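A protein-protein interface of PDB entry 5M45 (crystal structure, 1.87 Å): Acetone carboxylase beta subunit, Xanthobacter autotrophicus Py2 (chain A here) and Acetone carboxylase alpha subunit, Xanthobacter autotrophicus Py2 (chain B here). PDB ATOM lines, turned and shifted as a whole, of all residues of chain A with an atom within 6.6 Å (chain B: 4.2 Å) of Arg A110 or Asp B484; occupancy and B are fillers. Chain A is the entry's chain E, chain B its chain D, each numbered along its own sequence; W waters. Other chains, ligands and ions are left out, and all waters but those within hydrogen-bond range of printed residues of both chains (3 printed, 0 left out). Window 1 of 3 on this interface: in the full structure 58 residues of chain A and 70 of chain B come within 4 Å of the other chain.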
ATOM      1  N   PHE A 105      -4.534   8.912 -19.056  1.00  0.00           N
ATOM      2  CA  PHE A 105      -4.707  10.320 -18.577  1.00  0.00           C
ATOM      3  C   PHE A 105      -5.007  10.421 -17.086  1.00  0.00           C
ATOM      4  O   PHE A 105      -4.510  11.323 -16.426  1.00  0.00           O
ATOM      5  CB  PHE A 105      -5.637  11.188 -19.462  1.00  0.00           C
ATOM      6  CG  PHE A 105      -7.139  11.106 -19.173  1.00  0.00           C
ATOM      7  CD1 PHE A 105      -7.697  11.658 -18.015  1.00  0.00           C
ATOM      8  CD2 PHE A 105      -8.014  10.595 -20.149  1.00  0.00           C
ATOM      9  CE1 PHE A 105      -9.078  11.601 -17.780  1.00  0.00           C
ATOM     10  CE2 PHE A 105      -9.419  10.533 -19.937  1.00  0.00           C
ATOM     11  CZ  PHE A 105      -9.950  11.032 -18.748  1.00  0.00           C
ATOM     12  N   HIS A 106      -5.768   9.474 -16.566  1.00  0.00           N
ATOM     13  CA  HIS A 106      -6.179   9.454 -15.167  1.00  0.00           C
ATOM     14  C   HIS A 106      -4.970   9.287 -14.212  1.00  0.00           C
ATOM     15  O   HIS A 106      -4.786  10.086 -13.283  1.00  0.00           O
ATOM     16  CB  HIS A 106      -7.233   8.358 -14.952  1.00  0.00           C
ATOM     17  CG  HIS A 106      -7.624   8.157 -13.519  1.00  0.00           C
ATOM     18  ND1 HIS A 106      -8.183   9.168 -12.764  1.00  0.00           N
ATOM     19  CD2 HIS A 106      -7.469   7.098 -12.685  1.00  0.00           C
ATOM     20  CE1 HIS A 106      -8.393   8.725 -11.540  1.00  0.00           C
ATOM     21  NE2 HIS A 106      -7.964   7.480 -11.464  1.00  0.00           N
ATOM     22  N   ARG A 107      -4.154   8.277 -14.454  1.00  0.00           N
ATOM     23  CA  ARG A 107      -2.981   7.997 -13.613  1.00  0.00           C
ATOM     24  C   ARG A 107      -1.870   9.026 -13.743  1.00  0.00           C
ATOM     25  O   ARG A 107      -1.094   9.190 -12.814  1.00  0.00           O
ATOM     26  CB  ARG A 107      -2.469   6.571 -13.808  1.00  0.00           C
ATOM     27  CG  ARG A 107      -1.688   6.292 -15.076  1.00  0.00           C
ATOM     28  CD  ARG A 107      -1.435   4.814 -15.175  1.00  0.00           C
ATOM     29  NE  ARG A 107      -0.853   4.388 -16.456  1.00  0.00           N
ATOM     30  CZ  ARG A 107       0.306   3.758 -16.628  1.00  0.00           C
ATOM     31  NH1 ARG A 107       1.107   3.457 -15.585  1.00  0.00           N
ATOM     32  NH2 ARG A 107       0.651   3.388 -17.864  1.00  0.00           N
ATOM     33  N   MET A 108      -1.809   9.762 -14.862  1.00  0.00           N
ATOM     34  CA  MET A 108      -0.826  10.844 -15.008  1.00  0.00           C
ATOM     35  C   MET A 108      -1.120  12.038 -14.082  1.00  0.00           C
ATOM     36  O   MET A 108      -0.207  12.811 -13.785  1.00  0.00           O
ATOM     37  CB  MET A 108      -0.659  11.324 -16.460  1.00  0.00           C
ATOM     38  CG  MET A 108       0.032  10.312 -17.380  1.00  0.00           C
ATOM     39  SD  MET A 108       0.586  10.937 -19.035  1.00  0.00           S
ATOM     40  CE  MET A 108      -1.006  11.293 -19.700  1.00  0.00           C
ATOM     41  N   GLY A 109      -2.365  12.172 -13.618  1.00  0.00           N
ATOM     42  CA  GLY A 109      -2.719  13.219 -12.697  1.00  0.00           C
ATOM     43  C   GLY A 109      -2.539  14.634 -13.204  1.00  0.00           C
ATOM     44  O   GLY A 109      -2.417  15.584 -12.410  1.00  0.00           O
ATOM     45  N   ARG A 110      -2.546  14.776 -14.539  1.00  0.00           N
ATOM     46  CA  ARG A 110      -2.285  16.041 -15.216  1.00  0.00           C
ATOM     47  C   ARG A 110      -0.976  16.757 -14.772  1.00  0.00           C
ATOM     48  O   ARG A 110      -0.851  17.990 -14.967  1.00  0.00           O
ATOM     49  CB  ARG A 110      -3.485  16.968 -15.082  1.00  0.00           C
ATOM     50  CG  ARG A 110      -3.717  17.862 -16.312  1.00  0.00           C
ATOM     51  CD  ARG A 110      -4.919  18.789 -16.135  1.00  0.00           C
ATOM     52  NE  ARG A 110      -4.553  19.952 -15.311  1.00  0.00           N
ATOM     53  CZ  ARG A 110      -5.305  20.516 -14.362  1.00  0.00           C
ATOM     54  NH1 ARG A 110      -4.847  21.604 -13.707  1.00  0.00           N
ATOM     55  NH2 ARG A 110      -6.505  20.026 -14.022  1.00  0.00           N
ATOM     56  N   ALA A 111      -0.014  15.998 -14.208  1.00  0.00           N
ATOM     57  CA  ALA A 111       1.191  16.530 -13.526  1.00  0.00           C
ATOM     58  C   ALA A 111       0.903  17.254 -12.202  1.00  0.00           C
ATOM     59  O   ALA A 111       1.628  17.071 -11.208  1.00  0.00           O
ATOM     60  CB  ALA A 111       2.010  17.451 -14.436  1.00  0.00           C
ATOM     61  N   VAL A 112      -0.135  18.085 -12.210  1.00  0.00           N
ATOM     62  CA  VAL A 112      -0.468  18.960 -11.095  1.00  0.00           C
ATOM     63  C   VAL A 112      -0.682  18.193  -9.762  1.00  0.00           C
ATOM     64  O   VAL A 112      -0.290  18.705  -8.708  1.00  0.00           O
ATOM     65  CB  VAL A 112      -1.662  19.884 -11.476  1.00  0.00           C
ATOM     66  CG1 VAL A 112      -2.998  19.171 -11.333  1.00  0.00           C
ATOM     67  CG2 VAL A 112      -1.692  21.128 -10.657  1.00  0.00           C
ATOM     68  N   GLN A 113      -1.207  16.961  -9.824  1.00  0.00           N
ATOM     69  CA  GLN A 113      -1.432  16.161  -8.622  1.00  0.00           C
ATOM     70  C   GLN A 113      -0.145  15.730  -7.852  1.00  0.00           C
ATOM     71  O   GLN A 113      -0.262  15.227  -6.702  1.00  0.00           O
ATOM     72  CB  GLN A 113      -2.372  14.953  -8.898  1.00  0.00           C
ATOM     73  CG  GLN A 113      -3.809  15.407  -9.230  1.00  0.00           C
ATOM     74  CD  GLN A 113      -4.861  14.338  -9.528  1.00  0.00           C
ATOM     75  OE1 GLN A 113      -6.040  14.703  -9.730  1.00  0.00           O
ATOM     76  NE2 GLN A 113      -4.472  13.042  -9.614  1.00  0.00           N
ATOM     77  N   HIS A 115       2.006  17.988  -6.758  1.00  0.00           N
ATOM     78  CA  HIS A 115       2.323  19.122  -5.846  1.00  0.00           C
ATOM     79  C   HIS A 115       1.122  19.837  -5.225  1.00  0.00           C
ATOM     80  O   HIS A 115       1.268  20.909  -4.637  1.00  0.00           O
ATOM     81  CB  HIS A 115       3.270  20.123  -6.556  1.00  0.00           C
ATOM     82  CG  HIS A 115       2.790  20.591  -7.891  1.00  0.00           C
ATOM     83  ND1 HIS A 115       1.897  21.632  -8.037  1.00  0.00           N
ATOM     84  CD2 HIS A 115       3.078  20.169  -9.146  1.00  0.00           C
ATOM     85  CE1 HIS A 115       1.635  21.822  -9.323  1.00  0.00           C
ATOM     86  NE2 HIS A 115       2.341  20.959 -10.022  1.00  0.00           N
ATOM     87  N   TYR A 131       3.567  11.706  -6.469  1.00  0.00           N
ATOM     88  CA  TYR A 131       2.226  11.234  -6.897  1.00  0.00           C
ATOM     89  C   TYR A 131       1.694  10.179  -5.912  1.00  0.00           C
ATOM     90  O   TYR A 131       2.419   9.242  -5.591  1.00  0.00           O
ATOM     91  CB  TYR A 131       2.291  10.546  -8.286  1.00  0.00           C
ATOM     92  CG  TYR A 131       2.590  11.433  -9.472  1.00  0.00           C
ATOM     93  CD1 TYR A 131       1.625  12.280  -9.992  1.00  0.00           C
ATOM     94  CD2 TYR A 131       3.842  11.413 -10.088  1.00  0.00           C
ATOM     95  CE1 TYR A 131       1.899  13.086 -11.099  1.00  0.00           C
ATOM     96  CE2 TYR A 131       4.103  12.212 -11.199  1.00  0.00           C
ATOM     97  CZ  TYR A 131       3.122  13.044 -11.695  1.00  0.00           C
ATOM     98  OH  TYR A 131       3.379  13.856 -12.795  1.00  0.00           O
ATOM     99  N   LYS A 223     -13.363  19.843 -18.756  1.00  0.00           N
ATOM    100  CA  LYS A 223     -12.077  19.436 -18.106  1.00  0.00           C
ATOM    101  C   LYS A 223     -12.119  17.967 -17.734  1.00  0.00           C
ATOM    102  O   LYS A 223     -12.673  17.606 -16.686  1.00  0.00           O
ATOM    103  CB  LYS A 223     -11.690  20.279 -16.888  1.00  0.00           C
ATOM    104  CG  LYS A 223     -11.413  21.743 -17.211  1.00  0.00           C
ATOM    105  CD  LYS A 223     -10.963  22.519 -15.981  1.00  0.00           C
ATOM    106  CE  LYS A 223     -10.745  23.976 -16.319  1.00  0.00           C
ATOM    107  NZ  LYS A 223     -10.395  24.831 -15.127  1.00  0.00           N
ATOM    108  N   GLU A 224     -11.588  17.101 -18.599  1.00  0.00           N
ATOM    109  CA  GLU A 224     -11.719  15.667 -18.391  1.00  0.00           C
ATOM    110  C   GLU A 224     -11.065  15.162 -17.086  1.00  0.00           C
ATOM    111  O   GLU A 224     -11.559  14.193 -16.488  1.00  0.00           O
ATOM    112  CB  GLU A 224     -11.211  14.841 -19.578  1.00  0.00           C
ATOM    113  CG  GLU A 224      -9.683  14.755 -19.754  1.00  0.00           C
ATOM    114  CD  GLU A 224      -9.041  16.017 -20.373  1.00  0.00           C
ATOM    115  OE1 GLU A 224      -9.762  16.924 -20.861  1.00  0.00           O
ATOM    116  OE2 GLU A 224      -7.800  16.120 -20.368  1.00  0.00           O
ATOM    117  N   THR A 225      -9.983  15.789 -16.653  1.00  0.00           N
ATOM    118  CA  THR A 225      -9.300  15.313 -15.442  1.00  0.00           C
ATOM    119  C   THR A 225     -10.180  15.514 -14.179  1.00  0.00           C
ATOM    120  O   THR A 225     -10.469  14.559 -13.434  1.00  0.00           O
ATOM    121  CB  THR A 225      -7.894  15.913 -15.238  1.00  0.00           C
ATOM    122  OG1 THR A 225      -7.977  17.337 -15.132  1.00  0.00           O
ATOM    123  CG2 THR A 225      -6.987  15.578 -16.394  1.00  0.00           C
ATOM    124  N   HIS A 226     -10.669  16.743 -14.027  1.00  0.00           N
ATOM    125  CA  HIS A 226     -11.609  17.123 -12.979  1.00  0.00           C
ATOM    126  C   HIS A 226     -12.898  16.281 -13.027  1.00  0.00           C
ATOM    127  O   HIS A 226     -13.307  15.691 -12.005  1.00  0.00           O
ATOM    128  CB  HIS A 226     -11.990  18.621 -13.074  1.00  0.00           C
ATOM    129  CG  HIS A 226     -10.862  19.583 -12.806  1.00  0.00           C
ATOM    130  ND1 HIS A 226     -10.806  20.350 -11.663  1.00  0.00           N
ATOM    131  CD2 HIS A 226      -9.802  19.967 -13.567  1.00  0.00           C
ATOM    132  CE1 HIS A 226      -9.748  21.140 -11.716  1.00  0.00           C
ATOM    133  NE2 HIS A 226      -9.124  20.937 -12.857  1.00  0.00           N
ATOM    134  N   VAL A 337      -7.876  16.819  -8.443  1.00  0.00           N
ATOM    135  CA  VAL A 337      -8.650  17.851  -9.130  1.00  0.00           C
ATOM    136  C   VAL A 337     -10.124  17.396  -9.273  1.00  0.00           C
ATOM    137  O   VAL A 337     -10.378  16.246  -9.619  1.00  0.00           O
ATOM    138  CB  VAL A 337      -8.041  18.273 -10.483  1.00  0.00           C
ATOM    139  CG1 VAL A 337      -6.716  18.988 -10.252  1.00  0.00           C
ATOM    140  CG2 VAL A 337      -7.893  17.105 -11.474  1.00  0.00           C
ATOM    141  N   GLN B  86      -4.841  28.336 -17.012  1.00  0.00           N
ATOM    142  CA  GLN B  86      -4.785  26.981 -16.413  1.00  0.00           C
ATOM    143  C   GLN B  86      -3.370  26.633 -15.959  1.00  0.00           C
ATOM    144  O   GLN B  86      -3.159  26.282 -14.818  1.00  0.00           O
ATOM    145  CB  GLN B  86      -5.319  25.910 -17.390  1.00  0.00           C
ATOM    146  CG  GLN B  86      -5.352  24.556 -16.716  1.00  0.00           C
ATOM    147  CD  GLN B  86      -6.150  23.479 -17.437  1.00  0.00           C
ATOM    148  OE1 GLN B  86      -5.929  23.164 -18.611  1.00  0.00           O
ATOM    149  NE2 GLN B  86      -7.045  22.851 -16.684  1.00  0.00           N
ATOM    150  N   GLU B  87      -2.407  26.693 -16.860  1.00  0.00           N
ATOM    151  CA  GLU B  87      -0.990  26.367 -16.521  1.00  0.00           C
ATOM    152  C   GLU B  87      -0.320  27.334 -15.522  1.00  0.00           C
ATOM    153  O   GLU B  87       0.643  26.949 -14.902  1.00  0.00           O
ATOM    154  CB  GLU B  87      -0.122  26.297 -17.762  1.00  0.00           C
ATOM    155  CG  GLU B  87       0.057  24.930 -18.355  1.00  0.00           C
ATOM    156  CD  GLU B  87      -1.227  24.388 -18.819  1.00  0.00           C
ATOM    157  OE1 GLU B  87      -1.741  23.516 -18.090  1.00  0.00           O
ATOM    158  OE2 GLU B  87      -1.778  24.885 -19.850  1.00  0.00           O
ATOM    159  N   PHE B 456       1.883  24.131 -24.180  1.00  0.00           N
ATOM    160  CA  PHE B 456       2.647  24.013 -22.928  1.00  0.00           C
ATOM    161  C   PHE B 456       2.584  22.614 -22.278  1.00  0.00           C
ATOM    162  O   PHE B 456       2.762  22.460 -21.048  1.00  0.00           O
ATOM    163  CB  PHE B 456       2.293  25.164 -21.953  1.00  0.00           C
ATOM    164  CG  PHE B 456       3.224  26.364 -22.049  1.00  0.00           C
ATOM    165  CD1 PHE B 456       3.181  27.202 -23.149  1.00  0.00           C
ATOM    166  CD2 PHE B 456       4.134  26.647 -21.056  1.00  0.00           C
ATOM    167  CE1 PHE B 456       4.031  28.283 -23.259  1.00  0.00           C
ATOM    168  CE2 PHE B 456       4.993  27.724 -21.154  1.00  0.00           C
ATOM    169  CZ  PHE B 456       4.937  28.566 -22.250  1.00  0.00           C
ATOM    170  N   ALA B 459       5.603  21.857 -20.170  1.00  0.00           N
ATOM    171  CA  ALA B 459       5.684  22.192 -18.746  1.00  0.00           C
ATOM    172  C   ALA B 459       5.777  20.951 -17.862  1.00  0.00           C
ATOM    173  O   ALA B 459       6.085  21.104 -16.667  1.00  0.00           O
ATOM    174  CB  ALA B 459       4.473  23.029 -18.326  1.00  0.00           C
ATOM    175  N   GLU B 482       6.154  23.784 -10.570  1.00  0.00           N
ATOM    176  CA  GLU B 482       4.725  23.433 -10.462  1.00  0.00           C
ATOM    177  C   GLU B 482       4.178  23.001 -11.833  1.00  0.00           C
ATOM    178  O   GLU B 482       3.396  23.723 -12.473  1.00  0.00           O
ATOM    179  CB  GLU B 482       3.891  24.574  -9.853  1.00  0.00           C
ATOM    180  CG  GLU B 482       4.245  24.841  -8.391  1.00  0.00           C
ATOM    181  CD  GLU B 482       3.500  26.077  -7.817  1.00  0.00           C
ATOM    182  OE1 GLU B 482       2.289  25.993  -7.453  1.00  0.00           O
ATOM    183  OE2 GLU B 482       4.118  27.152  -7.730  1.00  0.00           O
ATOM    184  N   GLY B 483       4.580  21.824 -12.284  1.00  0.00           N
ATOM    185  CA  GLY B 483       4.200  21.377 -13.624  1.00  0.00           C
ATOM    186  C   GLY B 483       2.716  21.133 -13.799  1.00  0.00           C
ATOM    187  O   GLY B 483       2.026  20.753 -12.849  1.00  0.00           O
ATOM    188  N   ASP B 484       2.241  21.346 -15.026  1.00  0.00           N
ATOM    189  CA  ASP B 484       0.849  21.113 -15.408  1.00  0.00           C
ATOM    190  C   ASP B 484       0.813  20.879 -16.915  1.00  0.00           C
ATOM    191  O   ASP B 484       1.333  21.697 -17.649  1.00  0.00           O
ATOM    192  CB  ASP B 484       0.013  22.339 -15.040  1.00  0.00           C
ATOM    193  CG  ASP B 484      -1.554  22.054 -15.108  1.00  0.00           C
ATOM    194  OD1 ASP B 484      -1.987  21.077 -15.812  1.00  0.00           O
ATOM    195  OD2 ASP B 484      -2.331  22.817 -14.437  1.00  0.00           O
ATOM    196  N   MET B 485       0.252  19.752 -17.366  1.00  0.00           N
ATOM    197  CA  MET B 485       0.121  19.465 -18.813  1.00  0.00           C
ATOM    198  C   MET B 485      -1.142  20.064 -19.461  1.00  0.00           C
ATOM    199  O   MET B 485      -1.251  20.085 -20.705  1.00  0.00           O
ATOM    200  CB  MET B 485       0.200  17.959 -19.107  1.00  0.00           C
ATOM    201  CG  MET B 485      -0.895  17.121 -18.520  1.00  0.00           C
ATOM    202  SD  MET B 485      -0.811  15.361 -18.912  1.00  0.00           S
ATOM    203  CE  MET B 485       0.764  14.899 -18.159  1.00  0.00           C
ATOM    204  N   GLY B 486      -2.063  20.570 -18.643  1.00  0.00           N
ATOM    205  CA  GLY B 486      -3.355  21.074 -19.114  1.00  0.00           C
ATOM    206  C   GLY B 486      -4.323  19.972 -19.456  1.00  0.00           C
ATOM    207  O   GLY B 486      -3.895  18.813 -19.730  1.00  0.00           O
ATOM    208  N   ASP B 487      -5.609  20.318 -19.462  1.00  0.00           N
ATOM    209  CA  ASP B 487      -6.660  19.391 -19.898  1.00  0.00           C
ATOM    210  C   ASP B 487      -6.746  19.362 -21.420  1.00  0.00           C
ATOM    211  O   ASP B 487      -6.685  20.425 -22.078  1.00  0.00           O
ATOM    212  CB  ASP B 487      -8.036  19.798 -19.342  1.00  0.00           C
ATOM    213  CG  ASP B 487      -8.248  19.355 -17.905  1.00  0.00           C
ATOM    214  OD1 ASP B 487      -8.566  18.147 -17.702  1.00  0.00           O
ATOM    215  OD2 ASP B 487      -8.105  20.208 -16.963  1.00  0.00           O
HETATM  216  O   HOH W   1       0.819  23.825  -6.668  1.00  0.00           O
HETATM  217  O   HOH W   2      -3.728  13.888 -17.151  1.00  0.00           O
HETATM  218  O   HOH W   3      -8.096  23.463 -13.876  1.00  0.00           O
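The backbone carbonyl oxygen of Gly B483 sits at hydrogen-bond distance from the backbone NH of Val A112, 3.5 Å away. The backbone NH (N) of Met B485 sits at hydrogen-bond distance from the backbone carbonyl oxygen (O) of Arg A110, 3.2 Å away. OD1 of Asp B487 lies within hydrogen-bond range of OG1 of Thr A225 (2.8 Å). The side-chain carboxylate (OD1) of Asp B487 sits at hydrogen-bond distance from the backbone NH (N) of Glu A224 (3.3 Å). The guanidinium group of Arg A110 lies within salt-bridge range of the side-chain carboxylate of Asp B484. NE2 of His A115 lies within hydrogen-bond range of O of Gly B483 (2.9 Å). The guanidinium group (NH2) of Arg A110 lies within salt-bridge range of the side-chain carboxylate (OD2) of Asp B487.
Among the printed residues, pairs that only touch across the chains: His A115 with Glu B482 (3.3 Å), Arg A110 with Gly B486 (3.6 Å), Lys A223 with Asp B487 (3.6 Å), Ala A111 with Gly B483 (3.7 Å), Arg A110 with Gln B86 (3.7 Å), His A226 with Asp B487 (3.8 Å), Lys A223 with Gln B86 (3.9 Å) and Ala A111 with Asp B484 (3.9 Å).
Water W1 bridges the side-chain carboxylate of Glu B482 (2.7 Å) and a ring nitrogen (ND1) of His A115 (2.8 Å). Water W2 lies within hydrogen-bond range of O of Phe A105 (2.8 Å), N of Arg A110 (3.0 Å) and SD of Met B485 (3.7 Å). Water W3 lies within hydrogen-bond range of a ring nitrogen (NE2) of His A226 (2.9 Å), the side-chain amino group (NZ) of Lys A223 (3.0 Å) and the side-chain amide nitrogen (NE2) of Gln B86 (3.1 Å).
Of the 16 printed residues of chain A, 8 touch a printed residue of chain B. Hydrophobic or aromatic side chains of chain A that line the printed part of chain B: Ala A111, His A115 and His A226. Of the 10 printed residues of chain B, 7 touch a printed residue of chain A. Along chain B the printed residues that touch a printed residue of chain A span positions 86 to 487.
The side-chain carboxylate (OD2) of Asp B487 sits at hydrogen-bond distance from the side-chain amide nitrogen (NE2) of Gln B86 (2.9 Å). The side-chain carboxylate (OD1) of Asp B484 sits at hydrogen-bond distance from the backbone NH (N) of Gly B486. NH2 of Arg A110 is in hydrogen-bond range of NE2 of His A226 (3.0 Å). NH2 of Arg A110 is in hydrogen-bond range of OG1 of Thr A225 (3.3 Å). The side-chain carboxylate of Glu B87 sits at hydrogen-bond distance from the backbone NH of Gly B486, 3.0 Å away.
His A106 touches none of the printed residues of chain B. Tyr A131 touches none of the printed residues of chain B. Of the printed residues of chain B, His A226 touches Asp B487 (3.8 Å). Asp B484 touches two residues of chain A. Printed residues of chain A within 4 Å of Met B485: Arg A110. Of the printed residues of chain A, Gly B486 touches Arg A110. Of the printed residues of chain A, Asp B487 touches Arg A110, Lys A223, Glu A224, Thr A225 and His A226. The nearest printed residue of chain A that does not touch Gly B483 is Arg A110 (4.5 Å).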
